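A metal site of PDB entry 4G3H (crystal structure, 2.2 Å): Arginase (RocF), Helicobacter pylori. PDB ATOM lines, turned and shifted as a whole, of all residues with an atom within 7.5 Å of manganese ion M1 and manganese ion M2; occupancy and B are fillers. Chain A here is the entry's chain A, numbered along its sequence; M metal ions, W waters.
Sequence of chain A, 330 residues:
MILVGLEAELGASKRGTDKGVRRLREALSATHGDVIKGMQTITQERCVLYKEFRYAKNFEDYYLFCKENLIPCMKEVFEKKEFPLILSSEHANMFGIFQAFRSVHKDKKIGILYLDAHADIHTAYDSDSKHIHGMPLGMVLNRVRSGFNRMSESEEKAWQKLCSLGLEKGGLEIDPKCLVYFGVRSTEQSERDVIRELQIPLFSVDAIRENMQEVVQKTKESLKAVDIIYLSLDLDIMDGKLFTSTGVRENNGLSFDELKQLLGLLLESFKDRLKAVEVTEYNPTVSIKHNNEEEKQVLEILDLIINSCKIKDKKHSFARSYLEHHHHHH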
ATOM      1  N   GLU A  90     -28.413   1.284   4.276  1.00  0.00           N
ATOM      2  CA  GLU A  90     -28.057   1.018   5.587  1.00  0.00           C
ATOM      3  C   GLU A  90     -28.847  -0.053   6.266  1.00  0.00           C
ATOM      4  O   GLU A  90     -29.904  -0.090   6.062  1.00  0.00           O
ATOM      5  CB  GLU A  90     -27.880   2.301   6.389  1.00  0.00           C
ATOM      6  CG  GLU A  90     -28.981   3.138   6.576  1.00  0.00           C
ATOM      7  CD  GLU A  90     -28.626   4.432   7.299  1.00  0.00           C
ATOM      8  OE1 GLU A  90     -27.942   5.311   6.844  1.00  0.00           O
ATOM      9  OE2 GLU A  90     -29.114   4.598   8.312  1.00  0.00           O
ATOM     10  N   HIS A  91     -28.202  -0.968   6.979  1.00  0.00           N
ATOM     11  CA  HIS A  91     -28.950  -2.046   7.579  1.00  0.00           C
ATOM     12  C   HIS A  91     -30.122  -1.661   8.465  1.00  0.00           C
ATOM     13  O   HIS A  91     -31.091  -2.405   8.568  1.00  0.00           O
ATOM     14  CB  HIS A  91     -28.029  -2.995   8.345  1.00  0.00           C
ATOM     15  CG  HIS A  91     -28.260  -4.436   8.005  1.00  0.00           C
ATOM     16  ND1 HIS A  91     -29.409  -4.872   7.375  1.00  0.00           N
ATOM     17  CD2 HIS A  91     -27.488  -5.532   8.179  1.00  0.00           C
ATOM     18  CE1 HIS A  91     -29.328  -6.176   7.172  1.00  0.00           C
ATOM     19  NE2 HIS A  91     -28.171  -6.601   7.652  1.00  0.00           N
ATOM     20  N   ALA A  92     -30.062  -0.503   9.105  1.00  0.00           N
ATOM     21  CA  ALA A  92     -31.162  -0.079   9.965  1.00  0.00           C
ATOM     22  C   ALA A  92     -32.485  -0.038   9.205  1.00  0.00           C
ATOM     23  O   ALA A  92     -33.545  -0.234   9.797  1.00  0.00           O
ATOM     24  CB  ALA A  92     -30.864   1.287  10.586  1.00  0.00           C
ATOM     25  N   TYR A 114     -29.595 -14.079   7.555  1.00  0.00           N
ATOM     26  CA  TYR A 114     -28.935 -12.824   7.864  1.00  0.00           C
ATOM     27  C   TYR A 114     -27.418 -12.953   7.803  1.00  0.00           C
ATOM     28  O   TYR A 114     -26.799 -13.505   8.714  1.00  0.00           O
ATOM     29  CB  TYR A 114     -29.360 -12.384   9.276  1.00  0.00           C
ATOM     30  CG  TYR A 114     -29.345 -10.892   9.541  1.00  0.00           C
ATOM     31  CD1 TYR A 114     -30.391 -10.088   9.096  1.00  0.00           C
ATOM     32  CD2 TYR A 114     -28.304 -10.302  10.247  1.00  0.00           C
ATOM     33  CE1 TYR A 114     -30.404  -8.726   9.364  1.00  0.00           C
ATOM     34  CE2 TYR A 114     -28.304  -8.925  10.522  1.00  0.00           C
ATOM     35  CZ  TYR A 114     -29.372  -8.145  10.079  1.00  0.00           C
ATOM     36  OH  TYR A 114     -29.412  -6.796  10.345  1.00  0.00           O
ATOM     37  N   LEU A 115     -26.810 -12.452   6.736  1.00  0.00           N
ATOM     38  CA  LEU A 115     -25.352 -12.524   6.554  1.00  0.00           C
ATOM     39  C   LEU A 115     -24.804 -11.200   7.033  1.00  0.00           C
ATOM     40  O   LEU A 115     -25.049 -10.163   6.411  1.00  0.00           O
ATOM     41  CB  LEU A 115     -25.012 -12.769   5.088  1.00  0.00           C
ATOM     42  CG  LEU A 115     -25.368 -14.171   4.583  1.00  0.00           C
ATOM     43  CD1 LEU A 115     -26.882 -14.353   4.570  1.00  0.00           C
ATOM     44  CD2 LEU A 115     -24.790 -14.368   3.173  1.00  0.00           C
ATOM     45  N   ASP A 116     -24.026 -11.238   8.111  1.00  0.00           N
ATOM     46  CA  ASP A 116     -23.549  -9.995   8.706  1.00  0.00           C
ATOM     47  C   ASP A 116     -22.440 -10.264   9.723  1.00  0.00           C
ATOM     48  O   ASP A 116     -22.352 -11.355  10.285  1.00  0.00           O
ATOM     49  CB  ASP A 116     -24.747  -9.354   9.423  1.00  0.00           C
ATOM     50  CG  ASP A 116     -24.567  -7.891   9.726  1.00  0.00           C
ATOM     51  OD1 ASP A 116     -23.478  -7.459  10.169  1.00  0.00           O
ATOM     52  OD2 ASP A 116     -25.546  -7.160   9.540  1.00  0.00           O
ATOM     53  N   ALA A 117     -21.590  -9.267   9.944  1.00  0.00           N
ATOM     54  CA  ALA A 117     -20.524  -9.411  10.932  1.00  0.00           C
ATOM     55  C   ALA A 117     -21.157  -9.134  12.291  1.00  0.00           C
ATOM     56  O   ALA A 117     -20.592  -9.494  13.324  1.00  0.00           O
ATOM     57  CB  ALA A 117     -19.406  -8.404  10.647  1.00  0.00           C
ATOM     58  N   HIS A 118     -22.329  -8.494  12.282  1.00  0.00           N
ATOM     59  CA  HIS A 118     -23.043  -8.135  13.503  1.00  0.00           C
ATOM     60  C   HIS A 118     -24.420  -8.792  13.650  1.00  0.00           C
ATOM     61  O   HIS A 118     -25.025  -9.225  12.671  1.00  0.00           O
ATOM     62  CB  HIS A 118     -23.245  -6.615  13.566  1.00  0.00           C
ATOM     63  CG  HIS A 118     -22.023  -5.823  13.218  1.00  0.00           C
ATOM     64  ND1 HIS A 118     -21.746  -5.405  11.931  1.00  0.00           N
ATOM     65  CD2 HIS A 118     -20.966  -5.425  13.980  1.00  0.00           C
ATOM     66  CE1 HIS A 118     -20.575  -4.779  11.915  1.00  0.00           C
ATOM     67  NE2 HIS A 118     -20.092  -4.777  13.143  1.00  0.00           N
ATOM     68  N   ALA A 119     -24.896  -8.861  14.891  1.00  0.00           N
ATOM     69  CA  ALA A 119     -26.193  -9.453  15.186  1.00  0.00           C
ATOM     70  C   ALA A 119     -27.310  -8.422  15.021  1.00  0.00           C
ATOM     71  O   ALA A 119     -28.477  -8.771  14.795  1.00  0.00           O
ATOM     72  CB  ALA A 119     -26.201 -10.005  16.621  1.00  0.00           C
ATOM     73  N   ASP A 120     -26.956  -7.138  15.133  1.00  0.00           N
ATOM     74  CA  ASP A 120     -27.923  -6.053  14.984  1.00  0.00           C
ATOM     75  C   ASP A 120     -29.156  -6.189  15.877  1.00  0.00           C
ATOM     76  O   ASP A 120     -30.265  -5.833  15.467  1.00  0.00           O
ATOM     77  CB  ASP A 120     -28.380  -5.926  13.524  1.00  0.00           C
ATOM     78  CG  ASP A 120     -27.273  -5.457  12.588  1.00  0.00           C
ATOM     79  OD1 ASP A 120     -26.247  -4.943  13.074  1.00  0.00           O
ATOM     80  OD2 ASP A 120     -27.439  -5.599  11.350  1.00  0.00           O
ATOM     81  N   ILE A 132     -22.286   2.950  15.980  1.00  0.00           N
ATOM     82  CA  ILE A 132     -21.735   1.827  15.225  1.00  0.00           C
ATOM     83  C   ILE A 132     -22.794   1.161  14.355  1.00  0.00           C
ATOM     84  O   ILE A 132     -22.835   1.370  13.146  1.00  0.00           O
ATOM     85  CB  ILE A 132     -21.115   0.781  16.171  1.00  0.00           C
ATOM     86  CG1 ILE A 132     -19.921   1.391  16.909  1.00  0.00           C
ATOM     87  CG2 ILE A 132     -20.678  -0.447  15.367  1.00  0.00           C
ATOM     88  CD1 ILE A 132     -19.233   0.435  17.868  1.00  0.00           C
ATOM     89  N   HIS A 133     -23.649   0.339  14.971  1.00  0.00           N
ATOM     90  CA  HIS A 133     -24.697  -0.347  14.226  1.00  0.00           C
ATOM     91  C   HIS A 133     -26.055  -0.220  14.902  1.00  0.00           C
ATOM     92  O   HIS A 133     -26.144  -0.071  16.127  1.00  0.00           O
ATOM     93  CB  HIS A 133     -24.329  -1.825  14.045  1.00  0.00           C
ATOM     94  CG  HIS A 133     -24.392  -2.635  15.294  1.00  0.00           C
ATOM     95  ND1 HIS A 133     -25.580  -3.075  15.847  1.00  0.00           N
ATOM     96  CD2 HIS A 133     -23.413  -3.092  16.118  1.00  0.00           C
ATOM     97  CE1 HIS A 133     -25.324  -3.762  16.950  1.00  0.00           C
ATOM     98  NE2 HIS A 133     -24.015  -3.790  17.136  1.00  0.00           N
ATOM     99  N   GLY A 134     -27.114  -0.268  14.108  1.00  0.00           N
ATOM    100  CA  GLY A 134     -28.472  -0.160  14.625  1.00  0.00           C
ATOM    101  C   GLY A 134     -28.998  -1.442  15.263  1.00  0.00           C
ATOM    102  O   GLY A 134     -28.231  -2.341  15.611  1.00  0.00           O
ATOM    103  N   PRO A 136     -32.166  -3.254  13.964  1.00  0.00           N
ATOM    104  CA  PRO A 136     -33.360  -3.672  13.225  1.00  0.00           C
ATOM    105  C   PRO A 136     -33.909  -5.017  13.697  1.00  0.00           C
ATOM    106  O   PRO A 136     -35.121  -5.185  13.826  1.00  0.00           O
ATOM    107  CB  PRO A 136     -32.886  -3.703  11.771  1.00  0.00           C
ATOM    108  CG  PRO A 136     -31.431  -4.016  11.896  1.00  0.00           C
ATOM    109  CD  PRO A 136     -31.011  -3.139  13.061  1.00  0.00           C
ATOM    110  N   SER A 186     -19.089  -9.708  15.828  1.00  0.00           N
ATOM    111  CA  SER A 186     -18.928  -8.481  16.603  1.00  0.00           C
ATOM    112  C   SER A 186     -20.251  -8.160  17.261  1.00  0.00           C
ATOM    113  O   SER A 186     -21.178  -7.676  16.604  1.00  0.00           O
ATOM    114  CB  SER A 186     -18.478  -7.344  15.682  1.00  0.00           C
ATOM    115  OG  SER A 186     -18.266  -6.150  16.408  1.00  0.00           O
ATOM    116  N   SER A 232     -31.028 -11.255   3.934  1.00  0.00           N
ATOM    117  CA  SER A 232     -30.458  -9.935   4.166  1.00  0.00           C
ATOM    118  C   SER A 232     -28.944 -10.055   4.236  1.00  0.00           C
ATOM    119  O   SER A 232     -28.404 -10.697   5.123  1.00  0.00           O
ATOM    120  CB  SER A 232     -31.008  -9.345   5.460  1.00  0.00           C
ATOM    121  OG  SER A 232     -30.660  -7.975   5.573  1.00  0.00           O
ATOM    122  N   LEU A 233     -28.264  -9.418   3.276  1.00  0.00           N
ATOM    123  CA  LEU A 233     -26.812  -9.473   3.207  1.00  0.00           C
ATOM    124  C   LEU A 233     -26.125  -8.155   3.499  1.00  0.00           C
ATOM    125  O   LEU A 233     -26.332  -7.162   2.791  1.00  0.00           O
ATOM    126  CB  LEU A 233     -26.375  -9.966   1.810  1.00  0.00           C
ATOM    127  CG  LEU A 233     -24.896  -9.710   1.422  1.00  0.00           C
ATOM    128  CD1 LEU A 233     -23.962 -10.411   2.398  1.00  0.00           C
ATOM    129  CD2 LEU A 233     -24.626 -10.171   0.001  1.00  0.00           C
ATOM    130  N   ASP A 234     -25.282  -8.157   4.529  1.00  0.00           N
ATOM    131  CA  ASP A 234     -24.502  -6.989   4.933  1.00  0.00           C
ATOM    132  C   ASP A 234     -23.074  -7.309   4.464  1.00  0.00           C
ATOM    133  O   ASP A 234     -22.468  -8.280   4.902  1.00  0.00           O
ATOM    134  CB  ASP A 234     -24.519  -6.835   6.459  1.00  0.00           C
ATOM    135  CG  ASP A 234     -23.767  -5.594   6.929  1.00  0.00           C
ATOM    136  OD1 ASP A 234     -22.769  -5.178   6.280  1.00  0.00           O
ATOM    137  OD2 ASP A 234     -24.159  -5.040   7.973  1.00  0.00           O
ATOM    138  N   LEU A 235     -22.535  -6.473   3.586  1.00  0.00           N
ATOM    139  CA  LEU A 235     -21.209  -6.699   3.047  1.00  0.00           C
ATOM    140  C   LEU A 235     -20.067  -6.799   4.068  1.00  0.00           C
ATOM    141  O   LEU A 235     -18.999  -7.326   3.765  1.00  0.00           O
ATOM    142  CB  LEU A 235     -20.886  -5.625   1.998  1.00  0.00           C
ATOM    143  CG  LEU A 235     -21.805  -5.615   0.767  1.00  0.00           C
ATOM    144  CD1 LEU A 235     -21.581  -4.341  -0.044  1.00  0.00           C
ATOM    145  CD2 LEU A 235     -21.557  -6.854  -0.091  1.00  0.00           C
ATOM    146  N   ASP A 236     -20.284  -6.295   5.274  1.00  0.00           N
ATOM    147  CA  ASP A 236     -19.216  -6.373   6.262  1.00  0.00           C
ATOM    148  C   ASP A 236     -19.016  -7.800   6.775  1.00  0.00           C
ATOM    149  O   ASP A 236     -18.213  -8.032   7.689  1.00  0.00           O
ATOM    150  CB  ASP A 236     -19.443  -5.404   7.431  1.00  0.00           C
ATOM    151  CG  ASP A 236     -20.684  -5.728   8.249  1.00  0.00           C
ATOM    152  OD1 ASP A 236     -21.158  -6.884   8.225  1.00  0.00           O
ATOM    153  OD2 ASP A 236     -21.178  -4.811   8.930  1.00  0.00           O
ATOM    154  N   ILE A 237     -19.731  -8.763   6.195  1.00  0.00           N
ATOM    155  CA  ILE A 237     -19.544 -10.142   6.599  1.00  0.00           C
ATOM    156  C   ILE A 237     -18.179 -10.552   6.058  1.00  0.00           C
ATOM    157  O   ILE A 237     -17.507 -11.443   6.586  1.00  0.00           O
ATOM    158  CB  ILE A 237     -20.638 -11.073   6.029  1.00  0.00           C
ATOM    159  CG1 ILE A 237     -20.395 -12.513   6.494  1.00  0.00           C
ATOM    160  CG2 ILE A 237     -20.663 -10.991   4.520  1.00  0.00           C
ATOM    161  CD1 ILE A 237     -21.489 -13.506   6.131  1.00  0.00           C
ATOM    162  N   THR A 246     -17.107  -0.351   3.507  1.00  0.00           N
ATOM    163  CA  THR A 246     -18.225  -0.548   4.406  1.00  0.00           C
ATOM    164  C   THR A 246     -17.947   0.234   5.692  1.00  0.00           C
ATOM    165  O   THR A 246     -16.795   0.361   6.123  1.00  0.00           O
ATOM    166  CB  THR A 246     -18.438  -2.065   4.686  1.00  0.00           C
ATOM    167  OG1 THR A 246     -19.721  -2.261   5.303  1.00  0.00           O
ATOM    168  CG2 THR A 246     -17.359  -2.613   5.594  1.00  0.00           C
ATOM    169  N   VAL A 248     -18.601  -0.306   9.056  1.00  0.00           N
ATOM    170  CA  VAL A 248     -18.076  -0.949  10.266  1.00  0.00           C
ATOM    171  C   VAL A 248     -17.377  -2.252   9.907  1.00  0.00           C
ATOM    172  O   VAL A 248     -17.984  -3.320   9.940  1.00  0.00           O
ATOM    173  CB  VAL A 248     -19.211  -1.226  11.285  1.00  0.00           C
ATOM    174  CG1 VAL A 248     -18.631  -1.807  12.564  1.00  0.00           C
ATOM    175  CG2 VAL A 248     -19.966   0.064  11.578  1.00  0.00           C
ATOM    176  N   GLU A 250     -15.014  -5.453  10.284  1.00  0.00           N
ATOM    177  CA  GLU A 250     -14.671  -6.370  11.354  1.00  0.00           C
ATOM    178  C   GLU A 250     -13.691  -7.415  10.824  1.00  0.00           C
ATOM    179  O   GLU A 250     -13.915  -8.015   9.763  1.00  0.00           O
ATOM    180  CB  GLU A 250     -15.940  -7.043  11.887  1.00  0.00           C
ATOM    181  CG  GLU A 250     -17.009  -6.056  12.332  1.00  0.00           C
ATOM    182  CD  GLU A 250     -16.676  -5.403  13.667  1.00  0.00           C
ATOM    183  OE1 GLU A 250     -15.506  -5.485  14.098  1.00  0.00           O
ATOM    184  OE2 GLU A 250     -17.587  -4.793  14.275  1.00  0.00           O
ATOM    185  N   THR A 280     -26.863  -4.672   1.603  1.00  0.00           N
ATOM    186  CA  THR A 280     -26.691  -3.368   2.223  1.00  0.00           C
ATOM    187  C   THR A 280     -25.288  -3.057   2.746  1.00  0.00           C
ATOM    188  O   THR A 280     -24.402  -3.910   2.721  1.00  0.00           O
ATOM    189  CB  THR A 280     -27.681  -3.267   3.408  1.00  0.00           C
ATOM    190  OG1 THR A 280     -27.783  -1.915   3.869  1.00  0.00           O
ATOM    191  CG2 THR A 280     -27.201  -4.164   4.559  1.00  0.00           C
ATOM    192  N   GLU A 281     -25.117  -1.821   3.203  1.00  0.00           N
ATOM    193  CA  GLU A 281     -23.858  -1.346   3.757  1.00  0.00           C
ATOM    194  C   GLU A 281     -22.695  -1.259   2.781  1.00  0.00           C
ATOM    195  O   GLU A 281     -21.571  -1.678   3.098  1.00  0.00           O
ATOM    196  CB  GLU A 281     -23.460  -2.194   4.969  1.00  0.00           C
ATOM    197  CG  GLU A 281     -24.435  -2.101   6.159  1.00  0.00           C
ATOM    198  CD  GLU A 281     -24.539  -0.697   6.762  1.00  0.00           C
ATOM    199  OE1 GLU A 281     -23.602   0.110   6.571  1.00  0.00           O
ATOM    200  OE2 GLU A 281     -25.544  -0.399   7.426  1.00  0.00           O
HETATM  201 MN    MN M   1     -22.956  -5.300   9.951  1.00  0.00          MN
HETATM  202 MN    MN M   2     -25.872  -5.129   9.769  1.00  0.00          MN
HETATM  203  O   HOH W   1     -24.393  -3.102  10.722  1.00  0.00           O
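OD1 of Asp 236 lies within hydrogen-bond range of N of Ala 117 (3.0 Å).
The side-chain hydroxyl (OH) of Tyr 114 lies close to the side-chain carboxylate (OD2) of Asp 120, 2.5 Å away.
A ring nitrogen (ND1) of His 133 is in hydrogen-bond range of the side-chain carboxylate of Asp 120, 3.4 Å away.
The side-chain hydroxyl (OH) of Tyr 114 lies within hydrogen-bond range of a ring nitrogen (NE2) of His 91 (3.0 Å).
The side-chain carboxylate of Glu 281 sits at hydrogen-bond distance from the backbone NH of His 91, 2.8 Å away.
N of His 91 is in hydrogen-bond range of OG1 of Thr 280 (3.3 Å).
A ring nitrogen (NE2) of His 118 sits at hydrogen-bond distance from the side-chain carboxylate of Glu 250 (2.7 Å).
The backbone carbonyl oxygen of Leu 115 is in hydrogen-bond range of the backbone NH of Asp 234.
Within 4 Å of manganese ion M1: Asp 116, His 118, Asp 234 and Asp 236.
His 91 touches manganese ion M2 (CD2 to MN, 2.3 Å).
Tyr 114 touches manganese ion M2.
Five residues have an atom within 4 Å of manganese ion M2: His 91, Tyr 114, Asp 116, Asp 120 and Asp 234.
Manganese ion M1 is bound by the side-chain carboxylate (OD2) of Asp 236.
OD1 of Asp 116 is bound to manganese ion M1, at 2.2 Å.
A ring nitrogen (ND1) of His 118 binds manganese ion M1 (2.3 Å).
Manganese ion M1 is bound by the side-chain carboxylate (OD2) of Asp 234 (2.3 Å).
Manganese ion M1 has four donor atoms within binding distance.
Slightly farther from manganese ion M1 lies water W1 (2.7 Å).
Manganese ion M2 is bound by OD2 of Asp 116 (2.1 Å).
OD2 of Asp 120 binds manganese ion M2 (2.3 Å).
The side-chain carboxylate (OD2) of Asp 234 is bound to manganese ion M2.
Water W1 is bound to manganese ion M2, at 2.7 Å.
Manganese ion M2 has four donor atoms within binding distance.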
